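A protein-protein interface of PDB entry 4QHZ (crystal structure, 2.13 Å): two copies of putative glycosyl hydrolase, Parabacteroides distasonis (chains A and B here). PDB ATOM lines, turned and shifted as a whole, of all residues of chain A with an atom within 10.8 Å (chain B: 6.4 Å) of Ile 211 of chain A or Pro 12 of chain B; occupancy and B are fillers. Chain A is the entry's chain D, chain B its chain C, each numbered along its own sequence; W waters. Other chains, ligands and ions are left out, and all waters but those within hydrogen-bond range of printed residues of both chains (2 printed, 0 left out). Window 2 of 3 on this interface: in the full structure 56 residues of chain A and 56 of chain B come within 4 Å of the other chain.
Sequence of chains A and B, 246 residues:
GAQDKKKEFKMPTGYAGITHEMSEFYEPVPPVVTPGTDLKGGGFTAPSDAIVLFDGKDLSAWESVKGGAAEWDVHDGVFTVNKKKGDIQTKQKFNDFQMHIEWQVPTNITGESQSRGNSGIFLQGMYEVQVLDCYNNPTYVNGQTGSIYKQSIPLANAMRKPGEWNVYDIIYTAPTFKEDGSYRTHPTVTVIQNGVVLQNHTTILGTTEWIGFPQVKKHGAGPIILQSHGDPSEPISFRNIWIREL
The backbone carbonyl oxygen (O) of His 20 of chain B is in hydrogen-bond range of the side-chain amino group (NZ) of Lys 150 of chain A (2.9 Å).
The side-chain hydroxyl of Ser 23 of chain B sits at hydrogen-bond distance from the side-chain amino group of Lys 150 of chain A (3.1 Å).
The side-chain amide nitrogen (ND2) of Asn 142 of chain A lies within hydrogen-bond range of the backbone carbonyl oxygen (O) of Ser 23 of chain B (2.8 Å).
Among the printed residues, merely in contact across the chains: Trp 210 of chain A with His 20 of chain B, Ile 211 of chain A with Gly 14 of chain B, Ile 211 of chain A with Ile 18 of chain B, Ile 211 of chain A with Pro 12 of chain B, Trp 210 of chain A with Ser 23 of chain B, Ile 211 of chain A with His 20 of chain B, Gly 212 of chain A with Ile 18 of chain B and Trp 210 of chain A with Pro 12 of chain B.
Of the 11 printed residues of chain B, 5 touch a printed residue of chain A.
Hydrophobic or aromatic side chains of chain B that line the printed part of chain A: Pro 12, Ile 18 and His 20.
Of the 19 printed residues of chain A, 5 touch a printed residue of chain B.
Among the printed residues, 11 pairs touch across the chains.
Among the printed residues, no Asp or Glu carboxylate lies within 4 Å of a Lys or Arg side-chain nitrogen of the other chain.
A ring nitrogen (NE2) of His 20 of chain B lies close to the side-chain carboxylate (OE2) of Glu 21 of chain B, at 3.4 Å.
The side-chain amino group (NZ) of Lys 150 of chain A sits at hydrogen-bond distance from the backbone carbonyl oxygen (O) of Trp 210 of chain A (2.7 Å).
O of His 20 of chain B is in hydrogen-bond range of OG of Ser 23 of chain B (3.2 Å).
N of Lys 150 of chain A lies within hydrogen-bond range of O of Asn 142 of chain A (2.6 Å).
Of the printed residues of chain B, Asn 142 of chain A touches Ser 23 (2.8 Å).
Thr 208 of chain A touches none of the printed residues of chain B.
Of the printed residues of chain B, Ile 211 of chain A touches Pro 12, Gly 14, Ile 18 and His 20.
Of the printed residues of chain B, Gly 212 of chain A touches Ile 18.
No residue of chain A comes within 4 Å of Met 11 of chain B.
Of chain A, only Trp 210 and Ile 211 come within 4 Å of Pro 12 of chain B.
No residue of chain A comes within 4 Å of Thr 13 of chain B.
Of chain A, only Ile 211 comes within 4 Å of Gly 14 of chain B.
Of the printed residues of chain A, Ile 18 of chain B touches Ile 211 (3.6 Å) and Gly 212 (3.8 Å).
Printed residues of chain A within 4 Å of His 20 of chain B: Lys 150 (2.9 Å), Trp 210 (3.5 Å) and Ile 211 (3.7 Å).
Glu 21 of chain B touches none of the printed residues of chain A.
Printed residues of chain A within 4 Å of Ser 23 of chain B: Asn 142, Lys 150 and Trp 210.
The nearest residue of chain A that does not touch Pro 12 of chain B is Gly 212 of chain A (8.5 Å).
Water W1 lies within hydrogen-bond range of the side-chain hydroxyl of Ser 23 of chain B (2.6 Å), the backbone carbonyl oxygen of Gly 212 of chain A (2.7 Å) and the backbone carbonyl oxygen of Glu 209 of chain A (2.7 Å).
Water W2 lies within hydrogen-bond range of the side-chain hydroxyl of Ser 23 of chain B (2.7 Å), the backbone NH of Gly 212 of chain A (2.8 Å) and the backbone carbonyl oxygen of Thr 19 of chain B (2.8 Å).
No position is printed for both chains.
Of the 11 pairs that touch across the chains among the printed residues, none has its exchanged pair printed and touching as well.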
ATOM      1  N   GLN A 114     -11.761 -12.693  -0.380  1.00  0.00           N
ATOM      2  CA  GLN A 114     -13.063 -12.507  -1.024  1.00  0.00           C
ATOM      3  C   GLN A 114     -13.063 -11.456  -2.140  1.00  0.00           C
ATOM      4  O   GLN A 114     -14.065 -11.313  -2.840  1.00  0.00           O
ATOM      5  CB  GLN A 114     -14.128 -12.132   0.013  1.00  0.00           C
ATOM      6  CG  GLN A 114     -14.368 -13.193   1.074  1.00  0.00           C
ATOM      7  CD  GLN A 114     -15.095 -14.417   0.536  1.00  0.00           C
ATOM      8  OE1 GLN A 114     -16.170 -14.304  -0.056  1.00  0.00           O
ATOM      9  NE2 GLN A 114     -14.513 -15.600   0.747  1.00  0.00           N
ATOM     10  N   GLU A 128     -26.636 -18.631  -2.345  1.00  0.00           N
ATOM     11  CA  GLU A 128     -25.431 -18.453  -3.164  1.00  0.00           C
ATOM     12  C   GLU A 128     -24.517 -19.674  -3.167  1.00  0.00           C
ATOM     13  O   GLU A 128     -24.064 -20.124  -2.113  1.00  0.00           O
ATOM     14  CB  GLU A 128     -24.599 -17.238  -2.711  1.00  0.00           C
ATOM     15  CG  GLU A 128     -23.427 -16.950  -3.656  1.00  0.00           C
ATOM     16  CD  GLU A 128     -22.530 -15.796  -3.236  1.00  0.00           C
ATOM     17  OE1 GLU A 128     -22.643 -15.323  -2.088  1.00  0.00           O
ATOM     18  OE2 GLU A 128     -21.691 -15.379  -4.075  1.00  0.00           O
ATOM     19  N   TYR A 140     -11.685 -17.444   4.017  1.00  0.00           N
ATOM     20  CA  TYR A 140     -12.435 -18.220   5.012  1.00  0.00           C
ATOM     21  C   TYR A 140     -13.126 -19.374   4.303  1.00  0.00           C
ATOM     22  O   TYR A 140     -13.735 -19.199   3.247  1.00  0.00           O
ATOM     23  CB  TYR A 140     -13.414 -17.372   5.848  1.00  0.00           C
ATOM     24  CG  TYR A 140     -14.280 -16.358   5.133  1.00  0.00           C
ATOM     25  CD1 TYR A 140     -13.856 -15.038   4.985  1.00  0.00           C
ATOM     26  CD2 TYR A 140     -15.552 -16.696   4.675  1.00  0.00           C
ATOM     27  CE1 TYR A 140     -14.656 -14.090   4.362  1.00  0.00           C
ATOM     28  CE2 TYR A 140     -16.359 -15.758   4.049  1.00  0.00           C
ATOM     29  CZ  TYR A 140     -15.908 -14.457   3.894  1.00  0.00           C
ATOM     30  OH  TYR A 140     -16.703 -13.516   3.293  1.00  0.00           O
ATOM     31  N   ASN A 142     -15.594 -21.503   4.824  1.00  0.00           N
ATOM     32  CA  ASN A 142     -17.045 -21.581   4.640  1.00  0.00           C
ATOM     33  C   ASN A 142     -17.559 -20.564   3.608  1.00  0.00           C
ATOM     34  O   ASN A 142     -18.746 -20.536   3.322  1.00  0.00           O
ATOM     35  CB  ASN A 142     -17.789 -21.434   5.981  1.00  0.00           C
ATOM     36  CG  ASN A 142     -17.544 -20.095   6.658  1.00  0.00           C
ATOM     37  OD1 ASN A 142     -16.440 -19.546   6.609  1.00  0.00           O
ATOM     38  ND2 ASN A 142     -18.572 -19.569   7.311  1.00  0.00           N
ATOM     39  N   TYR A 149     -22.642 -20.329   0.541  1.00  0.00           N
ATOM     40  CA  TYR A 149     -21.897 -19.231   1.172  1.00  0.00           C
ATOM     41  C   TYR A 149     -22.155 -19.091   2.674  1.00  0.00           C
ATOM     42  O   TYR A 149     -23.281 -18.823   3.106  1.00  0.00           O
ATOM     43  CB  TYR A 149     -22.188 -17.909   0.452  1.00  0.00           C
ATOM     44  CG  TYR A 149     -21.400 -16.747   0.986  1.00  0.00           C
ATOM     45  CD1 TYR A 149     -20.023 -16.655   0.765  1.00  0.00           C
ATOM     46  CD2 TYR A 149     -22.017 -15.745   1.720  1.00  0.00           C
ATOM     47  CE1 TYR A 149     -19.289 -15.588   1.255  1.00  0.00           C
ATOM     48  CE2 TYR A 149     -21.293 -14.682   2.217  1.00  0.00           C
ATOM     49  CZ  TYR A 149     -19.931 -14.604   1.978  1.00  0.00           C
ATOM     50  OH  TYR A 149     -19.216 -13.538   2.483  1.00  0.00           O
ATOM     51  N   LYS A 150     -21.083 -19.306   3.442  1.00  0.00           N
ATOM     52  CA  LYS A 150     -21.056 -19.200   4.911  1.00  0.00           C
ATOM     53  C   LYS A 150     -21.936 -20.214   5.657  1.00  0.00           C
ATOM     54  O   LYS A 150     -22.261 -20.021   6.828  1.00  0.00           O
ATOM     55  CB  LYS A 150     -21.396 -17.760   5.358  1.00  0.00           C
ATOM     56  CG  LYS A 150     -20.245 -16.783   5.164  1.00  0.00           C
ATOM     57  CD  LYS A 150     -20.458 -15.491   5.931  1.00  0.00           C
ATOM     58  CE  LYS A 150     -19.212 -14.627   5.912  1.00  0.00           C
ATOM     59  NZ  LYS A 150     -19.305 -13.504   6.885  1.00  0.00           N
ATOM     60  N   GLN A 151     -22.313 -21.296   4.984  1.00  0.00           N
ATOM     61  CA  GLN A 151     -23.083 -22.370   5.613  1.00  0.00           C
ATOM     62  C   GLN A 151     -22.364 -23.707   5.540  1.00  0.00           C
ATOM     63  O   GLN A 151     -22.197 -24.366   6.561  1.00  0.00           O
ATOM     64  CB  GLN A 151     -24.441 -22.530   4.940  1.00  0.00           C
ATOM     65  CG  GLN A 151     -25.399 -21.385   5.193  1.00  0.00           C
ATOM     66  CD  GLN A 151     -26.737 -21.583   4.503  1.00  0.00           C
ATOM     67  OE1 GLN A 151     -27.135 -22.712   4.205  1.00  0.00           O
ATOM     68  NE2 GLN A 151     -27.427 -20.483   4.228  1.00  0.00           N
ATOM     69  N   GLY A 206     -31.010 -21.891   4.937  1.00  0.00           N
ATOM     70  CA  GLY A 206     -31.758 -20.652   4.775  1.00  0.00           C
ATOM     71  C   GLY A 206     -30.986 -19.758   3.830  1.00  0.00           C
ATOM     72  O   GLY A 206     -30.031 -20.207   3.200  1.00  0.00           O
ATOM     73  N   THR A 207     -31.383 -18.491   3.733  1.00  0.00           N
ATOM     74  CA  THR A 207     -30.670 -17.547   2.884  1.00  0.00           C
ATOM     75  C   THR A 207     -29.179 -17.516   3.232  1.00  0.00           C
ATOM     76  O   THR A 207     -28.805 -17.642   4.394  1.00  0.00           O
ATOM     77  CB  THR A 207     -31.213 -16.114   3.027  1.00  0.00           C
ATOM     78  OG1 THR A 207     -31.112 -15.700   4.393  1.00  0.00           O
ATOM     79  CG2 THR A 207     -32.666 -16.028   2.571  1.00  0.00           C
ATOM     80  N   THR A 208     -28.334 -17.356   2.220  1.00  0.00           N
ATOM     81  CA  THR A 208     -26.913 -17.146   2.456  1.00  0.00           C
ATOM     82  C   THR A 208     -26.700 -15.686   2.853  1.00  0.00           C
ATOM     83  O   THR A 208     -27.189 -14.782   2.182  1.00  0.00           O
ATOM     84  CB  THR A 208     -26.069 -17.521   1.229  1.00  0.00           C
ATOM     85  OG1 THR A 208     -26.599 -16.893   0.052  1.00  0.00           O
ATOM     86  CG2 THR A 208     -26.083 -19.024   1.053  1.00  0.00           C
ATOM     87  N   GLU A 209     -25.979 -15.469   3.950  1.00  0.00           N
ATOM     88  CA  GLU A 209     -25.849 -14.142   4.542  1.00  0.00           C
ATOM     89  C   GLU A 209     -24.400 -13.815   4.885  1.00  0.00           C
ATOM     90  O   GLU A 209     -23.686 -14.645   5.449  1.00  0.00           O
ATOM     91  CB  GLU A 209     -26.687 -14.057   5.815  1.00  0.00           C
ATOM     92  CG  GLU A 209     -28.177 -14.299   5.625  1.00  0.00           C
ATOM     93  CD  GLU A 209     -28.888 -13.165   4.901  1.00  0.00           C
ATOM     94  OE1 GLU A 209     -28.318 -12.060   4.791  1.00  0.00           O
ATOM     95  OE2 GLU A 209     -30.030 -13.379   4.448  1.00  0.00           O
ATOM     96  N   TRP A 210     -23.968 -12.611   4.524  1.00  0.00           N
ATOM     97  CA  TRP A 210     -22.646 -12.100   4.887  1.00  0.00           C
ATOM     98  C   TRP A 210     -22.588 -11.826   6.376  1.00  0.00           C
ATOM     99  O   TRP A 210     -21.549 -12.021   7.004  1.00  0.00           O
ATOM    100  CB  TRP A 210     -22.337 -10.820   4.098  1.00  0.00           C
ATOM    101  CG  TRP A 210     -20.967 -10.215   4.359  1.00  0.00           C
ATOM    102  CD1 TRP A 210     -19.768 -10.851   4.303  1.00  0.00           C
ATOM    103  CD2 TRP A 210     -20.682  -8.846   4.675  1.00  0.00           C
ATOM    104  NE1 TRP A 210     -18.751  -9.972   4.588  1.00  0.00           N
ATOM    105  CE2 TRP A 210     -19.287  -8.733   4.815  1.00  0.00           C
ATOM    106  CE3 TRP A 210     -21.474  -7.707   4.859  1.00  0.00           C
ATOM    107  CZ2 TRP A 210     -18.661  -7.530   5.128  1.00  0.00           C
ATOM    108  CZ3 TRP A 210     -20.849  -6.501   5.174  1.00  0.00           C
ATOM    109  CH2 TRP A 210     -19.456  -6.428   5.312  1.00  0.00           C
ATOM    110  N   ILE A 211     -23.708 -11.373   6.937  1.00  0.00           N
ATOM    111  CA  ILE A 211     -23.798 -11.068   8.359  1.00  0.00           C
ATOM    112  C   ILE A 211     -24.930 -11.858   9.003  1.00  0.00           C
ATOM    113  O   ILE A 211     -26.067 -11.811   8.535  1.00  0.00           O
ATOM    114  CB  ILE A 211     -24.024  -9.557   8.593  1.00  0.00           C
ATOM    115  CG1 ILE A 211     -22.762  -8.768   8.219  1.00  0.00           C
ATOM    116  CG2 ILE A 211     -24.415  -9.281  10.039  1.00  0.00           C
ATOM    117  CD1 ILE A 211     -22.942  -7.262   8.195  1.00  0.00           C
ATOM    118  N   GLY A 212     -24.614 -12.573  10.079  1.00  0.00           N
ATOM    119  CA  GLY A 212     -25.625 -13.242  10.883  1.00  0.00           C
ATOM    120  C   GLY A 212     -26.001 -14.632  10.412  1.00  0.00           C
ATOM    121  O   GLY A 212     -25.387 -15.188   9.496  1.00  0.00           O
ATOM    122  N   PHE A 213     -27.012 -15.199  11.067  1.00  0.00           N
ATOM    123  CA  PHE A 213     -27.463 -16.557  10.784  1.00  0.00           C
ATOM    124  C   PHE A 213     -28.284 -16.590   9.503  1.00  0.00           C
ATOM    125  O   PHE A 213     -28.889 -15.580   9.126  1.00  0.00           O
ATOM    126  CB  PHE A 213     -28.305 -17.092  11.938  1.00  0.00           C
ATOM    127  CG  PHE A 213     -27.515 -17.419  13.173  1.00  0.00           C
ATOM    128  CD1 PHE A 213     -27.033 -16.413  13.998  1.00  0.00           C
ATOM    129  CD2 PHE A 213     -27.263 -18.742  13.518  1.00  0.00           C
ATOM    130  CE1 PHE A 213     -26.308 -16.716  15.136  1.00  0.00           C
ATOM    131  CE2 PHE A 213     -26.544 -19.050  14.661  1.00  0.00           C
ATOM    132  CZ  PHE A 213     -26.065 -18.035  15.469  1.00  0.00           C
ATOM    133  N   PRO A 214     -28.322 -17.751   8.829  1.00  0.00           N
ATOM    134  CA  PRO A 214     -29.187 -17.874   7.651  1.00  0.00           C
ATOM    135  C   PRO A 214     -30.623 -17.523   7.995  1.00  0.00           C
ATOM    136  O   PRO A 214     -31.066 -17.811   9.101  1.00  0.00           O
ATOM    137  CB  PRO A 214     -29.067 -19.352   7.289  1.00  0.00           C
ATOM    138  CG  PRO A 214     -27.716 -19.743   7.779  1.00  0.00           C
ATOM    139  CD  PRO A 214     -27.524 -18.966   9.051  1.00  0.00           C
ATOM    140  N   GLN A 215     -31.331 -16.873   7.076  1.00  0.00           N
ATOM    141  CA  GLN A 215     -32.697 -16.446   7.350  1.00  0.00           C
ATOM    142  C   GLN A 215     -33.701 -17.343   6.648  1.00  0.00           C
ATOM    143  O   GLN A 215     -33.457 -17.831   5.542  1.00  0.00           O
ATOM    144  CB  GLN A 215     -32.892 -14.977   6.949  1.00  0.00           C
ATOM    145  CG  GLN A 215     -31.988 -14.052   7.750  1.00  0.00           C
ATOM    146  CD  GLN A 215     -32.214 -12.587   7.477  1.00  0.00           C
ATOM    147  OE1 GLN A 215     -31.255 -11.827   7.300  1.00  0.00           O
ATOM    148  NE2 GLN A 215     -33.474 -12.165   7.469  1.00  0.00           N
ATOM    149  N   VAL A 216     -34.830 -17.550   7.315  1.00  0.00           N
ATOM    150  CA  VAL A 216     -35.942 -18.317   6.785  1.00  0.00           C
ATOM    151  C   VAL A 216     -36.965 -17.352   6.193  1.00  0.00           C
ATOM    152  O   VAL A 216     -37.671 -16.671   6.927  1.00  0.00           O
ATOM    153  CB  VAL A 216     -36.587 -19.168   7.891  1.00  0.00           C
ATOM    154  CG1 VAL A 216     -37.829 -19.880   7.379  1.00  0.00           C
ATOM    155  CG2 VAL A 216     -35.579 -20.176   8.433  1.00  0.00           C
ATOM    156  N   MLY A 217     -37.026 -17.289   4.866  1.00  0.00           N
ATOM    157  CA  MLY A 217     -37.928 -16.374   4.156  1.00  0.00           C
ATOM    158  CB  MLY A 217     -37.128 -15.282   3.445  1.00  0.00           C
ATOM    159  CG  MLY A 217     -36.544 -14.234   4.386  1.00  0.00           C
ATOM    160  CD  MLY A 217     -35.783 -13.184   3.577  1.00  0.00           C
ATOM    161  CE  MLY A 217     -35.180 -12.119   4.485  1.00  0.00           C
ATOM    162  NZ  MLY A 217     -34.014 -11.359   3.982  1.00  0.00           N
ATOM    163  CH1 MLY A 217     -33.298 -11.808   2.752  1.00  0.00           C
ATOM    164  CH2 MLY A 217     -34.575 -10.026   3.764  1.00  0.00           C
ATOM    165  C   MLY A 217     -38.689 -17.135   3.112  1.00  0.00           C
ATOM    166  O   MLY A 217     -38.093 -17.631   2.161  1.00  0.00           O
ATOM    167  N   MLY B  10     -19.157   3.632   9.175  1.00  0.00           N
ATOM    168  CA  MLY B  10     -18.967   2.535  10.130  1.00  0.00           C
ATOM    169  CB  MLY B  10     -19.800   2.757  11.397  1.00  0.00           C
ATOM    170  CG  MLY B  10     -21.269   2.402  11.201  1.00  0.00           C
ATOM    171  CD  MLY B  10     -22.075   2.801  12.421  1.00  0.00           C
ATOM    172  CE  MLY B  10     -23.568   2.742  12.130  1.00  0.00           C
ATOM    173  NZ  MLY B  10     -24.047   1.408  11.726  1.00  0.00           N
ATOM    174  CH1 MLY B  10     -23.685   0.371  12.711  1.00  0.00           C
ATOM    175  CH2 MLY B  10     -25.513   1.472  11.588  1.00  0.00           C
ATOM    176  C   MLY B  10     -19.342   1.220   9.501  1.00  0.00           C
ATOM    177  O   MLY B  10     -20.128   1.165   8.548  1.00  0.00           O
ATOM    178  N   MET B  11     -18.775   0.148  10.046  1.00  0.00           N
ATOM    179  CA  MET B  11     -18.989  -1.195   9.521  1.00  0.00           C
ATOM    180  C   MET B  11     -20.386  -1.586   9.959  1.00  0.00           C
ATOM    181  O   MET B  11     -20.769  -1.340  11.105  1.00  0.00           O
ATOM    182  CB  MET B  11     -17.849  -2.103  10.005  1.00  0.00           C
ATOM    183  CG  MET B  11     -17.675  -3.375   9.160  1.00  0.00           C
ATOM    184  SD  MET B  11     -17.028  -3.080   7.307  1.00  0.00           S
ATOM    185  CE  MET B  11     -15.492  -4.303   7.358  1.00  0.00           C
ATOM    186  N   PRO B  12     -21.184  -2.164   9.041  1.00  0.00           N
ATOM    187  CA  PRO B  12     -22.528  -2.601   9.435  1.00  0.00           C
ATOM    188  C   PRO B  12     -22.515  -3.805  10.376  1.00  0.00           C
ATOM    189  O   PRO B  12     -21.588  -4.622  10.341  1.00  0.00           O
ATOM    190  CB  PRO B  12     -23.181  -2.984   8.106  1.00  0.00           C
ATOM    191  CG  PRO B  12     -22.041  -3.364   7.229  1.00  0.00           C
ATOM    192  CD  PRO B  12     -20.903  -2.469   7.628  1.00  0.00           C
ATOM    193  N   THR B  13     -23.528  -3.881  11.229  1.00  0.00           N
ATOM    194  CA  THR B  13     -23.713  -5.028  12.116  1.00  0.00           C
ATOM    195  C   THR B  13     -25.148  -5.530  11.992  1.00  0.00           C
ATOM    196  O   THR B  13     -26.034  -4.803  11.535  1.00  0.00           O
ATOM    197  CB  THR B  13     -23.400  -4.675  13.582  1.00  0.00           C
ATOM    198  OG1 THR B  13     -24.157  -3.524  13.969  1.00  0.00           O
ATOM    199  CG2 THR B  13     -21.921  -4.372  13.760  1.00  0.00           C
ATOM    200  N   GLY B  14     -25.362  -6.774  12.391  1.00  0.00           N
ATOM    201  CA  GLY B  14     -26.661  -7.425  12.240  1.00  0.00           C
ATOM    202  C   GLY B  14     -27.394  -7.540  13.560  1.00  0.00           C
ATOM    203  O   GLY B  14     -27.182  -6.740  14.475  1.00  0.00           O
ATOM    204  N   TYR B  15     -28.256  -8.549  13.653  1.00  0.00           N
ATOM    205  CA  TYR B  15     -29.081  -8.763  14.833  1.00  0.00           C
ATOM    206  C   TYR B  15     -28.232  -8.865  16.102  1.00  0.00           C
ATOM    207  O   TYR B  15     -27.276  -9.650  16.166  1.00  0.00           O
ATOM    208  CB  TYR B  15     -29.926 -10.025  14.660  1.00  0.00           C
ATOM    209  CG  TYR B  15     -30.767 -10.343  15.864  1.00  0.00           C
ATOM    210  CD1 TYR B  15     -31.979  -9.700  16.079  1.00  0.00           C
ATOM    211  CD2 TYR B  15     -30.345 -11.281  16.798  1.00  0.00           C
ATOM    212  CE1 TYR B  15     -32.751  -9.981  17.195  1.00  0.00           C
ATOM    213  CE2 TYR B  15     -31.107 -11.570  17.909  1.00  0.00           C
ATOM    214  CZ  TYR B  15     -32.306 -10.915  18.106  1.00  0.00           C
ATOM    215  OH  TYR B  15     -33.062 -11.211  19.213  1.00  0.00           O
ATOM    216  N   ILE B  18     -24.190  -8.635  15.781  1.00  0.00           N
ATOM    217  CA  ILE B  18     -23.337  -9.644  15.161  1.00  0.00           C
ATOM    218  C   ILE B  18     -22.576  -9.027  13.982  1.00  0.00           C
ATOM    219  O   ILE B  18     -23.134  -8.221  13.231  1.00  0.00           O
ATOM    220  CB  ILE B  18     -24.144 -10.895  14.717  1.00  0.00           C
ATOM    221  CG1 ILE B  18     -23.198 -12.056  14.398  1.00  0.00           C
ATOM    222  CG2 ILE B  18     -25.043 -10.578  13.527  1.00  0.00           C
ATOM    223  CD1 ILE B  18     -23.870 -13.409  14.367  1.00  0.00           C
ATOM    224  N   THR B  19     -21.302  -9.398  13.854  1.00  0.00           N
ATOM    225  CA  THR B  19     -20.411  -8.870  12.822  1.00  0.00           C
ATOM    226  C   THR B  19     -20.114  -9.950  11.789  1.00  0.00           C
ATOM    227  O   THR B  19     -20.233 -11.148  12.079  1.00  0.00           O
ATOM    228  CB  THR B  19     -19.064  -8.404  13.406  1.00  0.00           C
ATOM    229  OG1 THR B  19     -18.379  -9.525  13.979  1.00  0.00           O
ATOM    230  CG2 THR B  19     -19.250  -7.335  14.477  1.00  0.00           C
ATOM    231  N   HIS B  20     -19.700  -9.538  10.594  1.00  0.00           N
ATOM    232  CA  HIS B  20     -19.445 -10.497   9.517  1.00  0.00           C
ATOM    233  C   HIS B  20     -18.322 -11.489   9.876  1.00  0.00           C
ATOM    234  O   HIS B  20     -18.368 -12.645   9.458  1.00  0.00           O
ATOM    235  CB  HIS B  20     -19.166  -9.780   8.182  1.00  0.00           C
ATOM    236  CG  HIS B  20     -17.859  -9.058   8.123  1.00  0.00           C
ATOM    237  ND1 HIS B  20     -16.712  -9.639   7.631  1.00  0.00           N
ATOM    238  CD2 HIS B  20     -17.524  -7.791   8.459  1.00  0.00           C
ATOM    239  CE1 HIS B  20     -15.720  -8.765   7.685  1.00  0.00           C
ATOM    240  NE2 HIS B  20     -16.186  -7.637   8.186  1.00  0.00           N
ATOM    241  N   GLU B  21     -17.345 -11.043  10.669  1.00  0.00           N
ATOM    242  CA  GLU B  21     -16.222 -11.887  11.085  1.00  0.00           C
ATOM    243  C   GLU B  21     -16.661 -13.099  11.904  1.00  0.00           C
ATOM    244  O   GLU B  21     -15.998 -14.135  11.881  1.00  0.00           O
ATOM    245  CB  GLU B  21     -15.196 -11.091  11.909  1.00  0.00           C
ATOM    246  CG  GLU B  21     -14.403 -10.058  11.115  1.00  0.00           C
ATOM    247  CD  GLU B  21     -14.973  -8.654  11.219  1.00  0.00           C
ATOM    248  OE1 GLU B  21     -16.177  -8.509  11.523  1.00  0.00           O
ATOM    249  OE2 GLU B  21     -14.212  -7.690  10.995  1.00  0.00           O
ATOM    250  N   SER B  23     -18.954 -15.105  11.487  1.00  0.00           N
ATOM    251  CA  SER B  23     -19.358 -16.240  10.661  1.00  0.00           C
ATOM    252  C   SER B  23     -18.310 -16.556   9.590  1.00  0.00           C
ATOM    253  O   SER B  23     -18.645 -17.070   8.531  1.00  0.00           O
ATOM    254  CB  SER B  23     -20.735 -15.985  10.025  1.00  0.00           C
ATOM    255  OG  SER B  23     -20.745 -14.799   9.252  1.00  0.00           O
HETATM  256  O   HOH W   1     -23.086 -15.107   8.083  1.00  0.00           O
HETATM  257  O   HOH W   2     -22.003 -13.040  10.933  1.00  0.00           O
